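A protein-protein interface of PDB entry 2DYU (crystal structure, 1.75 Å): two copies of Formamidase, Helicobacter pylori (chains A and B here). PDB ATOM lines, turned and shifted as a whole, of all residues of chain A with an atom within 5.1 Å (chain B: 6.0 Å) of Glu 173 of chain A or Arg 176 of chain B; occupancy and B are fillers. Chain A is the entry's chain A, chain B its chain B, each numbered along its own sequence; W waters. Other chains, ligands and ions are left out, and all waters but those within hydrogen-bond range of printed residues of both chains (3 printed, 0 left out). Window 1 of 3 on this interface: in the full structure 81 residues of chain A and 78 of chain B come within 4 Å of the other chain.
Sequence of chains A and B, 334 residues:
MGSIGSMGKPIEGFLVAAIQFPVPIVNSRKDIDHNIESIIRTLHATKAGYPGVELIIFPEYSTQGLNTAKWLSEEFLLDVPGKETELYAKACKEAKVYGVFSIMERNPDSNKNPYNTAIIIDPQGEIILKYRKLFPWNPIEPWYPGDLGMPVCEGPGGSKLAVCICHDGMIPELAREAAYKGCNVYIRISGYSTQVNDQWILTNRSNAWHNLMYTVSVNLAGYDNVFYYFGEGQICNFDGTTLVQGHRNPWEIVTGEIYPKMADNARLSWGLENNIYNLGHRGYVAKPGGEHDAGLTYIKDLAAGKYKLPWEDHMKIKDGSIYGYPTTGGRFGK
NH1 of Arg 176 of chain B sits at hydrogen-bond distance from O of His 210 of chain B (2.9 Å).
OH of Tyr 298 of chain A is in hydrogen-bond range of OE2 of Glu 173 of chain A, 2.7 Å away.
The guanidinium group (NH1) of Arg 176 of chain B sits at hydrogen-bond distance from the side-chain amide oxygen (OD1) of Asn 211 of chain B (3.0 Å).
The side-chain carboxylate (OE2) of Glu 173 of chain B sits at hydrogen-bond distance from the side-chain hydroxyl (OH) of Tyr 298 of chain B (2.8 Å).
Water W3 lies within hydrogen-bond range of OE2 of Glu 173 of chain B, O of Pro 172 of chain A and N of Glu 173 of chain A.
Water W2 lies within hydrogen-bond range of the guanidinium group of Arg 176 of chain B (2.8 Å), the backbone carbonyl oxygen of Met 170 of chain A (2.9 Å) and the backbone carbonyl oxygen of His 210 of chain B (2.9 Å).
Water W1 lies within hydrogen-bond range of the side-chain carboxylate of Glu 173 of chain A (2.8 Å), the backbone carbonyl oxygen of Pro 172 of chain B (3.2 Å) and the backbone NH of Glu 173 of chain B (3.3 Å).
Printed residues of chain B within 4 Å of Glu 173 of chain A: Arg 176, Leu 279, Leu 296 and Tyr 298.
Arg 176 of chain B touches just these residues of chain A: Pro 172 (3.4 Å), Glu 173 (2.8 Å), Tyr 298 (3.4 Å) and Tyr 307 (3.96 Å).
Printed residues of chain A within 4 Å of Asn 275 of chain B: Met 170 and Ile 171.
Of the printed residues of chain A, Pro 172 of chain B touches Arg 176.
Ala 175 of chain B touches none of the printed residues of chain A.
Leu 174 of chain B touches none of the printed residues of chain A.
The nearest residue of chain B that does not touch Glu 173 of chain A is Ile 299 of chain B (4.4 Å).
The nearest residue of chain A that does not touch Arg 176 of chain B is Ile 171 of chain A (4.6 Å).
The nearest printed residue of chain A that does not touch Leu 296 of chain B is Ile 171 of chain A (5.7 Å).
Pro 172 of chain A touches Arg 176 of chain B, and with the chains exchanged Arg 176 of chain A touches Pro 172 of chain B.
Glu 173 of chain A touches Arg 176 of chain B, and with the chains exchanged Arg 176 of chain A touches Glu 173 of chain B.
Arg 176 of chain A touches Tyr 298 of chain B, and with the chains exchanged Tyr 298 of chain A touches Arg 176 of chain B.
Glu 177 of chain A touches Tyr 298 of chain B, and with the chains exchanged Tyr 298 of chain A touches Glu 177 of chain B.
8 positions are printed for both chains.
The backbone carbonyl oxygen (O) of Met 170 of chain A is in hydrogen-bond range of a ring nitrogen (ND1) of His 210 of chain B.
The backbone carbonyl oxygen of Ile 276 of chain B sits at hydrogen-bond distance from the side-chain hydroxyl of Tyr 307 of chain A (2.7 Å).
OE1 of Glu 177 of chain A lies within hydrogen-bond range of N of Tyr 298 of chain B, at 2.9 Å.
The side-chain carboxylate (OE1) of Glu 177 of chain B is in hydrogen-bond range of the backbone NH (N) of Tyr 298 of chain A (3.0 Å).
The guanidinium group (NH2) of Arg 176 of chain A is in salt-bridge range of the side-chain carboxylate (OE1) of Glu 173 of chain B.
NE of Arg 176 of chain B is in salt-bridge range of OE2 of Glu 173 of chain A, 2.8 Å away.
Printed residues of chain B that touch a printed residue of chain A: Pro 172, Glu 173, Arg 176, Glu 177, Tyr 180, His 210, Asn 275, Ile 276, Leu 279, Leu 296 and Tyr 298.
Of the 10 printed residues of chain A, 9 touch a printed residue of chain B.
Along chain A the printed residues that touch a printed residue of chain B span positions 170 to 307.
Among the printed residues, pairs that only touch across the chains: Met 170 of chain A with Asn 275 of chain B, Ile 171 of chain A with Asn 275 of chain B, Ile 171 of chain A with Leu 279 of chain B, Pro 172 of chain A with Arg 176 of chain B, Pro 172 of chain A with His 210 of chain B, Glu 173 of chain A with Leu 279 of chain B, Glu 173 of chain A with Leu 296 of chain B, Glu 173 of chain A with Tyr 298 of chain B, Leu 174 of chain A with Leu 296 of chain B, Arg 176 of chain A with Pro 172 of chain B, Arg 176 of chain A with Tyr 298 of chain B, Glu 177 of chain A with Leu 296 of chain B, Tyr 298 of chain A with Glu 173 of chain B, Tyr 298 of chain A with Arg 176 of chain B, Tyr 298 of chain A with Tyr 180 of chain B, Tyr 307 of chain A with Arg 176 of chain B, Tyr 307 of chain A with Tyr 180 of chain B and Tyr 307 of chain A with Leu 279 of chain B.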
ATOM      1  N   MET A 170     -27.555  14.552 -11.464  1.00  0.00           N
ATOM      2  CA  MET A 170     -27.647  14.783 -12.912  1.00  0.00           C
ATOM      3  C   MET A 170     -27.024  13.659 -13.748  1.00  0.00           C
ATOM      4  O   MET A 170     -27.101  13.673 -14.977  1.00  0.00           O
ATOM      5  CB  MET A 170     -26.948  16.100 -13.294  1.00  0.00           C
ATOM      6  CG  MET A 170     -27.548  17.366 -12.668  1.00  0.00           C
ATOM      7  SD  MET A 170     -29.327  17.496 -12.972  1.00  0.00           S
ATOM      8  CE  MET A 170     -29.461  16.414 -14.381  1.00  0.00           C
ATOM      9  N   ILE A 171     -26.389  12.710 -13.070  1.00  0.00           N
ATOM     10  CA  ILE A 171     -25.656  11.631 -13.716  1.00  0.00           C
ATOM     11  C   ILE A 171     -26.453  10.336 -13.571  1.00  0.00           C
ATOM     12  O   ILE A 171     -26.506   9.748 -12.483  1.00  0.00           O
ATOM     13  CB  ILE A 171     -24.240  11.455 -13.093  1.00  0.00           C
ATOM     14  CG1 ILE A 171     -23.499  12.796 -12.988  1.00  0.00           C
ATOM     15  CG2 ILE A 171     -23.417  10.422 -13.880  1.00  0.00           C
ATOM     16  CD1 ILE A 171     -23.175  13.463 -14.341  1.00  0.00           C
ATOM     17  N   PRO A 172     -27.120   9.907 -14.654  1.00  0.00           N
ATOM     18  CA  PRO A 172     -28.013   8.754 -14.547  1.00  0.00           C
ATOM     19  C   PRO A 172     -27.264   7.471 -14.224  1.00  0.00           C
ATOM     20  O   PRO A 172     -27.823   6.580 -13.588  1.00  0.00           O
ATOM     21  CB  PRO A 172     -28.670   8.682 -15.936  1.00  0.00           C
ATOM     22  CG  PRO A 172     -27.707   9.377 -16.858  1.00  0.00           C
ATOM     23  CD  PRO A 172     -27.087  10.463 -16.019  1.00  0.00           C
ATOM     24  N   GLU A 173     -26.006   7.382 -14.660  1.00  0.00           N
ATOM     25  CA  GLU A 173     -25.179   6.218 -14.346  1.00  0.00           C
ATOM     26  C   GLU A 173     -25.027   6.028 -12.836  1.00  0.00           C
ATOM     27  O   GLU A 173     -24.929   4.906 -12.354  1.00  0.00           O
ATOM     28  CB  GLU A 173     -23.804   6.335 -15.018  1.00  0.00           C
ATOM     29  CG  GLU A 173     -23.816   6.170 -16.546  1.00  0.00           C
ATOM     30  CD  GLU A 173     -24.163   7.443 -17.316  1.00  0.00           C
ATOM     31  OE1 GLU A 173     -24.417   8.505 -16.703  1.00  0.00           O
ATOM     32  OE2 GLU A 173     -24.160   7.383 -18.560  1.00  0.00           O
ATOM     33  N   LEU A 174     -25.003   7.131 -12.096  1.00  0.00           N
ATOM     34  CA  LEU A 174     -24.823   7.063 -10.659  1.00  0.00           C
ATOM     35  C   LEU A 174     -26.078   6.539  -9.963  1.00  0.00           C
ATOM     36  O   LEU A 174     -25.988   5.795  -8.998  1.00  0.00           O
ATOM     37  CB  LEU A 174     -24.448   8.434 -10.090  1.00  0.00           C
ATOM     38  CG  LEU A 174     -24.090   8.449  -8.612  1.00  0.00           C
ATOM     39  CD1 LEU A 174     -22.974   7.448  -8.343  1.00  0.00           C
ATOM     40  CD2 LEU A 174     -23.681   9.849  -8.200  1.00  0.00           C
ATOM     41  N   ALA A 175     -27.246   6.950 -10.446  1.00  0.00           N
ATOM     42  CA  ALA A 175     -28.505   6.414  -9.924  1.00  0.00           C
ATOM     43  C   ALA A 175     -28.585   4.922 -10.227  1.00  0.00           C
ATOM     44  O   ALA A 175     -29.034   4.117  -9.388  1.00  0.00           O
ATOM     45  CB  ALA A 175     -29.698   7.154 -10.520  1.00  0.00           C
ATOM     46  N   ARG A 176     -28.129   4.551 -11.422  1.00  0.00           N
ATOM     47  CA  ARG A 176     -28.070   3.144 -11.824  1.00  0.00           C
ATOM     48  C   ARG A 176     -27.157   2.354 -10.886  1.00  0.00           C
ATOM     49  O   ARG A 176     -27.500   1.251 -10.450  1.00  0.00           O
ATOM     50  CB  ARG A 176     -27.586   2.998 -13.274  1.00  0.00           C
ATOM     51  CG  ARG A 176     -27.547   1.557 -13.751  1.00  0.00           C
ATOM     52  CD  ARG A 176     -28.935   1.082 -14.107  1.00  0.00           C
ATOM     53  NE  ARG A 176     -29.315   1.501 -15.451  1.00  0.00           N
ATOM     54  CZ  ARG A 176     -30.567   1.512 -15.898  1.00  0.00           C
ATOM     55  NH1 ARG A 176     -31.563   1.175 -15.081  1.00  0.00           N
ATOM     56  NH2 ARG A 176     -30.827   1.871 -17.153  1.00  0.00           N
ATOM     57  N   GLU A 177     -26.005   2.931 -10.560  1.00  0.00           N
ATOM     58  CA  GLU A 177     -25.064   2.307  -9.625  1.00  0.00           C
ATOM     59  C   GLU A 177     -25.667   2.048  -8.245  1.00  0.00           C
ATOM     60  O   GLU A 177     -25.470   0.969  -7.663  1.00  0.00           O
ATOM     61  CB  GLU A 177     -23.794   3.162  -9.492  1.00  0.00           C
ATOM     62  CG  GLU A 177     -22.751   2.629  -8.493  1.00  0.00           C
ATOM     63  CD  GLU A 177     -22.107   1.307  -8.910  1.00  0.00           C
ATOM     64  OE1 GLU A 177     -22.402   0.792 -10.010  1.00  0.00           O
ATOM     65  OE2 GLU A 177     -21.299   0.774  -8.117  1.00  0.00           O
ATOM     66  N   TYR A 298     -19.000   3.428 -24.869  1.00  0.00           N
ATOM     67  CA  TYR A 298     -18.719   4.339 -23.758  1.00  0.00           C
ATOM     68  C   TYR A 298     -18.579   3.602 -22.436  1.00  0.00           C
ATOM     69  O   TYR A 298     -17.804   4.015 -21.577  1.00  0.00           O
ATOM     70  CB  TYR A 298     -19.754   5.451 -23.673  1.00  0.00           C
ATOM     71  CG  TYR A 298     -20.857   5.288 -22.649  1.00  0.00           C
ATOM     72  CD1 TYR A 298     -20.674   5.698 -21.332  1.00  0.00           C
ATOM     73  CD2 TYR A 298     -22.113   4.788 -23.021  1.00  0.00           C
ATOM     74  CE1 TYR A 298     -21.693   5.583 -20.392  1.00  0.00           C
ATOM     75  CE2 TYR A 298     -23.140   4.669 -22.088  1.00  0.00           C
ATOM     76  CZ  TYR A 298     -22.923   5.075 -20.783  1.00  0.00           C
ATOM     77  OH  TYR A 298     -23.932   4.978 -19.860  1.00  0.00           O
ATOM     78  N   TYR A 307     -12.763   7.144 -21.050  1.00  0.00           N
ATOM     79  CA  TYR A 307     -13.910   7.876 -21.597  1.00  0.00           C
ATOM     80  C   TYR A 307     -13.408   9.198 -22.161  1.00  0.00           C
ATOM     81  O   TYR A 307     -12.734   9.973 -21.471  1.00  0.00           O
ATOM     82  CB  TYR A 307     -14.934   8.092 -20.481  1.00  0.00           C
ATOM     83  CG  TYR A 307     -16.209   8.861 -20.790  1.00  0.00           C
ATOM     84  CD1 TYR A 307     -17.409   8.187 -20.995  1.00  0.00           C
ATOM     85  CD2 TYR A 307     -16.237  10.255 -20.758  1.00  0.00           C
ATOM     86  CE1 TYR A 307     -18.597   8.876 -21.213  1.00  0.00           C
ATOM     87  CE2 TYR A 307     -17.426  10.955 -20.975  1.00  0.00           C
ATOM     88  CZ  TYR A 307     -18.599  10.255 -21.207  1.00  0.00           C
ATOM     89  OH  TYR A 307     -19.783  10.938 -21.411  1.00  0.00           O
ATOM     90  N   ILE B 171     -33.835   3.425 -21.725  1.00  0.00           N
ATOM     91  CA  ILE B 171     -32.497   3.047 -21.284  1.00  0.00           C
ATOM     92  C   ILE B 171     -31.550   4.218 -21.503  1.00  0.00           C
ATOM     93  O   ILE B 171     -31.159   4.476 -22.642  1.00  0.00           O
ATOM     94  CB  ILE B 171     -31.948   1.834 -22.086  1.00  0.00           C
ATOM     95  CG1 ILE B 171     -32.936   0.658 -22.098  1.00  0.00           C
ATOM     96  CG2 ILE B 171     -30.585   1.398 -21.532  1.00  0.00           C
ATOM     97  CD1 ILE B 171     -33.051  -0.088 -20.795  1.00  0.00           C
ATOM     98  N   PRO B 172     -31.178   4.936 -20.420  1.00  0.00           N
ATOM     99  CA  PRO B 172     -30.363   6.140 -20.556  1.00  0.00           C
ATOM    100  C   PRO B 172     -28.976   5.833 -21.114  1.00  0.00           C
ATOM    101  O   PRO B 172     -28.380   6.687 -21.756  1.00  0.00           O
ATOM    102  CB  PRO B 172     -30.272   6.674 -19.117  1.00  0.00           C
ATOM    103  CG  PRO B 172     -30.486   5.471 -18.253  1.00  0.00           C
ATOM    104  CD  PRO B 172     -31.519   4.668 -19.010  1.00  0.00           C
ATOM    105  N   GLU B 173     -28.484   4.618 -20.884  1.00  0.00           N
ATOM    106  CA  GLU B 173     -27.170   4.217 -21.392  1.00  0.00           C
ATOM    107  C   GLU B 173     -27.107   4.282 -22.922  1.00  0.00           C
ATOM    108  O   GLU B 173     -26.047   4.528 -23.498  1.00  0.00           O
ATOM    109  CB  GLU B 173     -26.812   2.798 -20.911  1.00  0.00           C
ATOM    110  CG  GLU B 173     -26.402   2.692 -19.432  1.00  0.00           C
ATOM    111  CD  GLU B 173     -27.584   2.597 -18.478  1.00  0.00           C
ATOM    112  OE1 GLU B 173     -28.752   2.523 -18.950  1.00  0.00           O
ATOM    113  OE2 GLU B 173     -27.332   2.590 -17.250  1.00  0.00           O
ATOM    114  N   LEU B 174     -28.244   4.043 -23.577  1.00  0.00           N
ATOM    115  CA  LEU B 174     -28.325   4.074 -25.044  1.00  0.00           C
ATOM    116  C   LEU B 174     -28.275   5.492 -25.592  1.00  0.00           C
ATOM    117  O   LEU B 174     -27.666   5.738 -26.640  1.00  0.00           O
ATOM    118  CB  LEU B 174     -29.602   3.383 -25.520  1.00  0.00           C
ATOM    119  CG  LEU B 174     -29.494   2.090 -26.332  1.00  0.00           C
ATOM    120  CD1 LEU B 174     -28.263   1.245 -25.987  1.00  0.00           C
ATOM    121  CD2 LEU B 174     -30.773   1.282 -26.177  1.00  0.00           C
ATOM    122  N   ALA B 175     -28.926   6.421 -24.883  1.00  0.00           N
ATOM    123  CA  ALA B 175     -28.845   7.837 -25.213  1.00  0.00           C
ATOM    124  C   ALA B 175     -27.418   8.331 -25.023  1.00  0.00           C
ATOM    125  O   ALA B 175     -26.898   9.064 -25.857  1.00  0.00           O
ATOM    126  CB  ALA B 175     -29.806   8.651 -24.362  1.00  0.00           C
ATOM    127  N   ARG B 176     -26.785   7.901 -23.936  1.00  0.00           N
ATOM    128  CA  ARG B 176     -25.389   8.250 -23.686  1.00  0.00           C
ATOM    129  C   ARG B 176     -24.491   7.730 -24.813  1.00  0.00           C
ATOM    130  O   ARG B 176     -23.629   8.456 -25.304  1.00  0.00           O
ATOM    131  CB  ARG B 176     -24.921   7.711 -22.330  1.00  0.00           C
ATOM    132  CG  ARG B 176     -23.498   8.167 -21.942  1.00  0.00           C
ATOM    133  CD  ARG B 176     -23.505   9.602 -21.502  1.00  0.00           C
ATOM    134  NE  ARG B 176     -23.907   9.740 -20.100  1.00  0.00           N
ATOM    135  CZ  ARG B 176     -24.311  10.880 -19.559  1.00  0.00           C
ATOM    136  NH1 ARG B 176     -24.399  11.968 -20.310  1.00  0.00           N
ATOM    137  NH2 ARG B 176     -24.622  10.925 -18.268  1.00  0.00           N
ATOM    138  N   GLU B 177     -24.708   6.488 -25.225  1.00  0.00           N
ATOM    139  CA  GLU B 177     -23.891   5.892 -26.287  1.00  0.00           C
ATOM    140  C   GLU B 177     -23.996   6.685 -27.592  1.00  0.00           C
ATOM    141  O   GLU B 177     -22.981   6.957 -28.240  1.00  0.00           O
ATOM    142  CB  GLU B 177     -24.253   4.420 -26.503  1.00  0.00           C
ATOM    143  CG  GLU B 177     -23.515   3.750 -27.663  1.00  0.00           C
ATOM    144  CD  GLU B 177     -22.022   3.603 -27.413  1.00  0.00           C
ATOM    145  OE1 GLU B 177     -21.567   3.887 -26.290  1.00  0.00           O
ATOM    146  OE2 GLU B 177     -21.299   3.183 -28.342  1.00  0.00           O
ATOM    147  N   ALA B 178     -25.218   7.070 -27.959  1.00  0.00           N
ATOM    148  CA  ALA B 178     -25.442   7.896 -29.145  1.00  0.00           C
ATOM    149  C   ALA B 178     -24.645   9.189 -29.052  1.00  0.00           C
ATOM    150  O   ALA B 178     -23.886   9.521 -29.961  1.00  0.00           O
ATOM    151  CB  ALA B 178     -26.928   8.203 -29.312  1.00  0.00           C
ATOM    152  N   ALA B 179     -24.818   9.902 -27.938  1.00  0.00           N
ATOM    153  CA  ALA B 179     -24.138  11.175 -27.694  1.00  0.00           C
ATOM    154  C   ALA B 179     -22.622  11.019 -27.710  1.00  0.00           C
ATOM    155  O   ALA B 179     -21.914  11.844 -28.284  1.00  0.00           O
ATOM    156  CB  ALA B 179     -24.586  11.753 -26.370  1.00  0.00           C
ATOM    157  N   TYR B 180     -22.144   9.944 -27.090  1.00  0.00           N
ATOM    158  CA  TYR B 180     -20.716   9.647 -26.997  1.00  0.00           C
ATOM    159  C   TYR B 180     -20.086   9.522 -28.380  1.00  0.00           C
ATOM    160  O   TYR B 180     -18.894   9.793 -28.556  1.00  0.00           O
ATOM    161  CB  TYR B 180     -20.511   8.344 -26.225  1.00  0.00           C
ATOM    162  CG  TYR B 180     -19.076   8.053 -25.847  1.00  0.00           C
ATOM    163  CD1 TYR B 180     -18.412   8.833 -24.901  1.00  0.00           C
ATOM    164  CD2 TYR B 180     -18.388   6.984 -26.423  1.00  0.00           C
ATOM    165  CE1 TYR B 180     -17.095   8.568 -24.542  1.00  0.00           C
ATOM    166  CE2 TYR B 180     -17.074   6.706 -26.064  1.00  0.00           C
ATOM    167  CZ  TYR B 180     -16.433   7.504 -25.132  1.00  0.00           C
ATOM    168  OH  TYR B 180     -15.129   7.229 -24.778  1.00  0.00           O
ATOM    169  N   LYS B 181     -20.891   9.093 -29.343  1.00  0.00           N
ATOM    170  CA  LYS B 181     -20.450   8.925 -30.724  1.00  0.00           C
ATOM    171  C   LYS B 181     -20.757  10.147 -31.590  1.00  0.00           C
ATOM    172  O   LYS B 181     -20.557  10.118 -32.815  1.00  0.00           O
ATOM    173  CB  LYS B 181     -21.104   7.676 -31.322  1.00  0.00           C
ATOM    174  CG  LYS B 181     -20.512   6.339 -30.865  1.00  0.00           C
ATOM    175  CD  LYS B 181     -21.472   5.223 -31.219  1.00  0.00           C
ATOM    176  CE  LYS B 181     -20.749   4.027 -31.779  1.00  0.00           C
ATOM    177  NZ  LYS B 181     -21.681   3.164 -32.561  1.00  0.00           N
ATOM    178  N   HIS B 210     -29.637  14.990 -20.235  1.00  0.00           N
ATOM    179  CA  HIS B 210     -28.495  14.213 -19.741  1.00  0.00           C
ATOM    180  C   HIS B 210     -27.312  14.360 -20.680  1.00  0.00           C
ATOM    181  O   HIS B 210     -26.160  14.314 -20.255  1.00  0.00           O
ATOM    182  CB  HIS B 210     -28.831  12.720 -19.679  1.00  0.00           C
ATOM    183  CG  HIS B 210     -29.619  12.302 -18.470  1.00  0.00           C
ATOM    184  ND1 HIS B 210     -29.572  12.967 -17.263  1.00  0.00           N
ATOM    185  CD2 HIS B 210     -30.437  11.239 -18.280  1.00  0.00           C
ATOM    186  CE1 HIS B 210     -30.339  12.339 -16.385  1.00  0.00           C
ATOM    187  NE2 HIS B 210     -30.874  11.289 -16.978  1.00  0.00           N
ATOM    188  N   ASN B 211     -27.610  14.506 -21.968  1.00  0.00           N
ATOM    189  CA  ASN B 211     -26.578  14.452 -23.006  1.00  0.00           C
ATOM    190  C   ASN B 211     -26.382  15.729 -23.801  1.00  0.00           C
ATOM    191  O   ASN B 211     -25.598  15.755 -24.750  1.00  0.00           O
ATOM    192  CB  ASN B 211     -26.899  13.307 -23.954  1.00  0.00           C
ATOM    193  CG  ASN B 211     -26.880  11.983 -23.249  1.00  0.00           C
ATOM    194  OD1 ASN B 211     -25.815  11.489 -22.885  1.00  0.00           O
ATOM    195  ND2 ASN B 211     -28.062  11.414 -23.007  1.00  0.00           N
ATOM    196  N   MET B 213     -28.477  17.166 -25.965  1.00  0.00           N
ATOM    197  CA  MET B 213     -28.855  16.979 -27.370  1.00  0.00           C
ATOM    198  C   MET B 213     -30.351  17.115 -27.512  1.00  0.00           C
ATOM    199  O   MET B 213     -31.079  16.992 -26.527  1.00  0.00           O
ATOM    200  CB  MET B 213     -28.420  15.600 -27.886  1.00  0.00           C
ATOM    201  CG  MET B 213     -29.092  14.391 -27.211  1.00  0.00           C
ATOM    202  SD  MET B 213     -28.265  12.839 -27.623  1.00  0.00           S
ATOM    203  CE  MET B 213     -29.173  11.678 -26.612  1.00  0.00           C
ATOM    204  N   ASN B 275     -22.803  17.844 -17.964  1.00  0.00           N
ATOM    205  CA  ASN B 275     -22.809  16.569 -17.268  1.00  0.00           C
ATOM    206  C   ASN B 275     -22.154  15.442 -18.065  1.00  0.00           C
ATOM    207  O   ASN B 275     -21.491  14.573 -17.500  1.00  0.00           O
ATOM    208  CB  ASN B 275     -24.246  16.231 -16.874  1.00  0.00           C
ATOM    209  CG  ASN B 275     -24.800  17.228 -15.876  1.00  0.00           C
ATOM    210  OD1 ASN B 275     -25.812  17.892 -16.116  1.00  0.00           O
ATOM    211  ND2 ASN B 275     -24.121  17.355 -14.758  1.00  0.00           N
ATOM    212  N   ILE B 276     -22.324  15.479 -19.383  1.00  0.00           N
ATOM    213  CA  ILE B 276     -21.731  14.449 -20.237  1.00  0.00           C
ATOM    214  C   ILE B 276     -20.193  14.437 -20.157  1.00  0.00           C
ATOM    215  O   ILE B 276     -19.570  13.386 -20.231  1.00  0.00           O
ATOM    216  CB  ILE B 276     -22.256  14.549 -21.694  1.00  0.00           C
ATOM    217  CG1 ILE B 276     -21.807  13.334 -22.511  1.00  0.00           C
ATOM    218  CG2 ILE B 276     -21.887  15.891 -22.338  1.00  0.00           C
ATOM    219  CD1 ILE B 276     -22.544  13.162 -23.824  1.00  0.00           C
ATOM    220  N   LEU B 279     -19.095  13.108 -16.417  1.00  0.00           N
ATOM    221  CA  LEU B 279     -19.126  11.648 -16.246  1.00  0.00           C
ATOM    222  C   LEU B 279     -17.732  11.012 -16.256  1.00  0.00           C
ATOM    223  O   LEU B 279     -17.434  10.132 -15.444  1.00  0.00           O
ATOM    224  CB  LEU B 279     -19.998  10.990 -17.324  1.00  0.00           C
ATOM    225  CG  LEU B 279     -20.083   9.457 -17.308  1.00  0.00           C
ATOM    226  CD1 LEU B 279     -20.502   8.935 -15.932  1.00  0.00           C
ATOM    227  CD2 LEU B 279     -21.034   8.987 -18.388  1.00  0.00           C
ATOM    228  N   LEU B 296     -17.939   3.326 -10.368  1.00  0.00           N
ATOM    229  CA  LEU B 296     -19.190   2.600 -10.532  1.00  0.00           C
ATOM    230  C   LEU B 296     -18.974   1.126 -10.902  1.00  0.00           C
ATOM    231  O   LEU B 296     -18.475   0.805 -11.984  1.00  0.00           O
ATOM    232  CB  LEU B 296     -20.058   3.293 -11.594  1.00  0.00           C
ATOM    233  CG  LEU B 296     -20.194   4.821 -11.532  1.00  0.00           C
ATOM    234  CD1 LEU B 296     -21.098   5.335 -12.650  1.00  0.00           C
ATOM    235  CD2 LEU B 296     -20.720   5.264 -10.170  1.00  0.00           C
ATOM    236  N   TYR B 298     -21.206  -1.221 -11.677  1.00  0.00           N
ATOM    237  CA  TYR B 298     -22.035  -1.786 -12.744  1.00  0.00           C
ATOM    238  C   TYR B 298     -21.444  -1.548 -14.125  1.00  0.00           C
ATOM    239  O   TYR B 298     -21.625  -2.362 -15.026  1.00  0.00           O
ATOM    240  CB  TYR B 298     -23.474  -1.272 -12.675  1.00  0.00           C
ATOM    241  CG  TYR B 298     -23.820  -0.127 -13.601  1.00  0.00           C
ATOM    242  CD1 TYR B 298     -24.311  -0.362 -14.889  1.00  0.00           C
ATOM    243  CD2 TYR B 298     -23.700   1.193 -13.174  1.00  0.00           C
ATOM    244  CE1 TYR B 298     -24.648   0.697 -15.737  1.00  0.00           C
ATOM    245  CE2 TYR B 298     -24.042   2.242 -13.997  1.00  0.00           C
ATOM    246  CZ  TYR B 298     -24.515   1.997 -15.274  1.00  0.00           C
ATOM    247  OH  TYR B 298     -24.855   3.057 -16.077  1.00  0.00           O
ATOM    248  N   ILE B 299     -20.757  -0.416 -14.283  1.00  0.00           N
ATOM    249  CA  ILE B 299     -20.079  -0.076 -15.523  1.00  0.00           C
ATOM    250  C   ILE B 299     -18.995  -1.103 -15.811  1.00  0.00           C
ATOM    251  O   ILE B 299     -18.903  -1.621 -16.920  1.00  0.00           O
ATOM    252  CB  ILE B 299     -19.428   1.324 -15.429  1.00  0.00           C
ATOM    253  CG1 ILE B 299     -20.508   2.414 -15.343  1.00  0.00           C
ATOM    254  CG2 ILE B 299     -18.458   1.564 -16.598  1.00  0.00           C
ATOM    255  CD1 ILE B 299     -21.337   2.559 -16.583  1.00  0.00           C
HETATM  256  O   HOH W   1     -26.910   6.746 -18.934  1.00  0.00           O
HETATM  257  O   HOH W   2     -25.809  13.372 -17.500  1.00  0.00           O
HETATM  258  O   HOH W   3     -27.705   5.258 -16.459  1.00  0.00           O
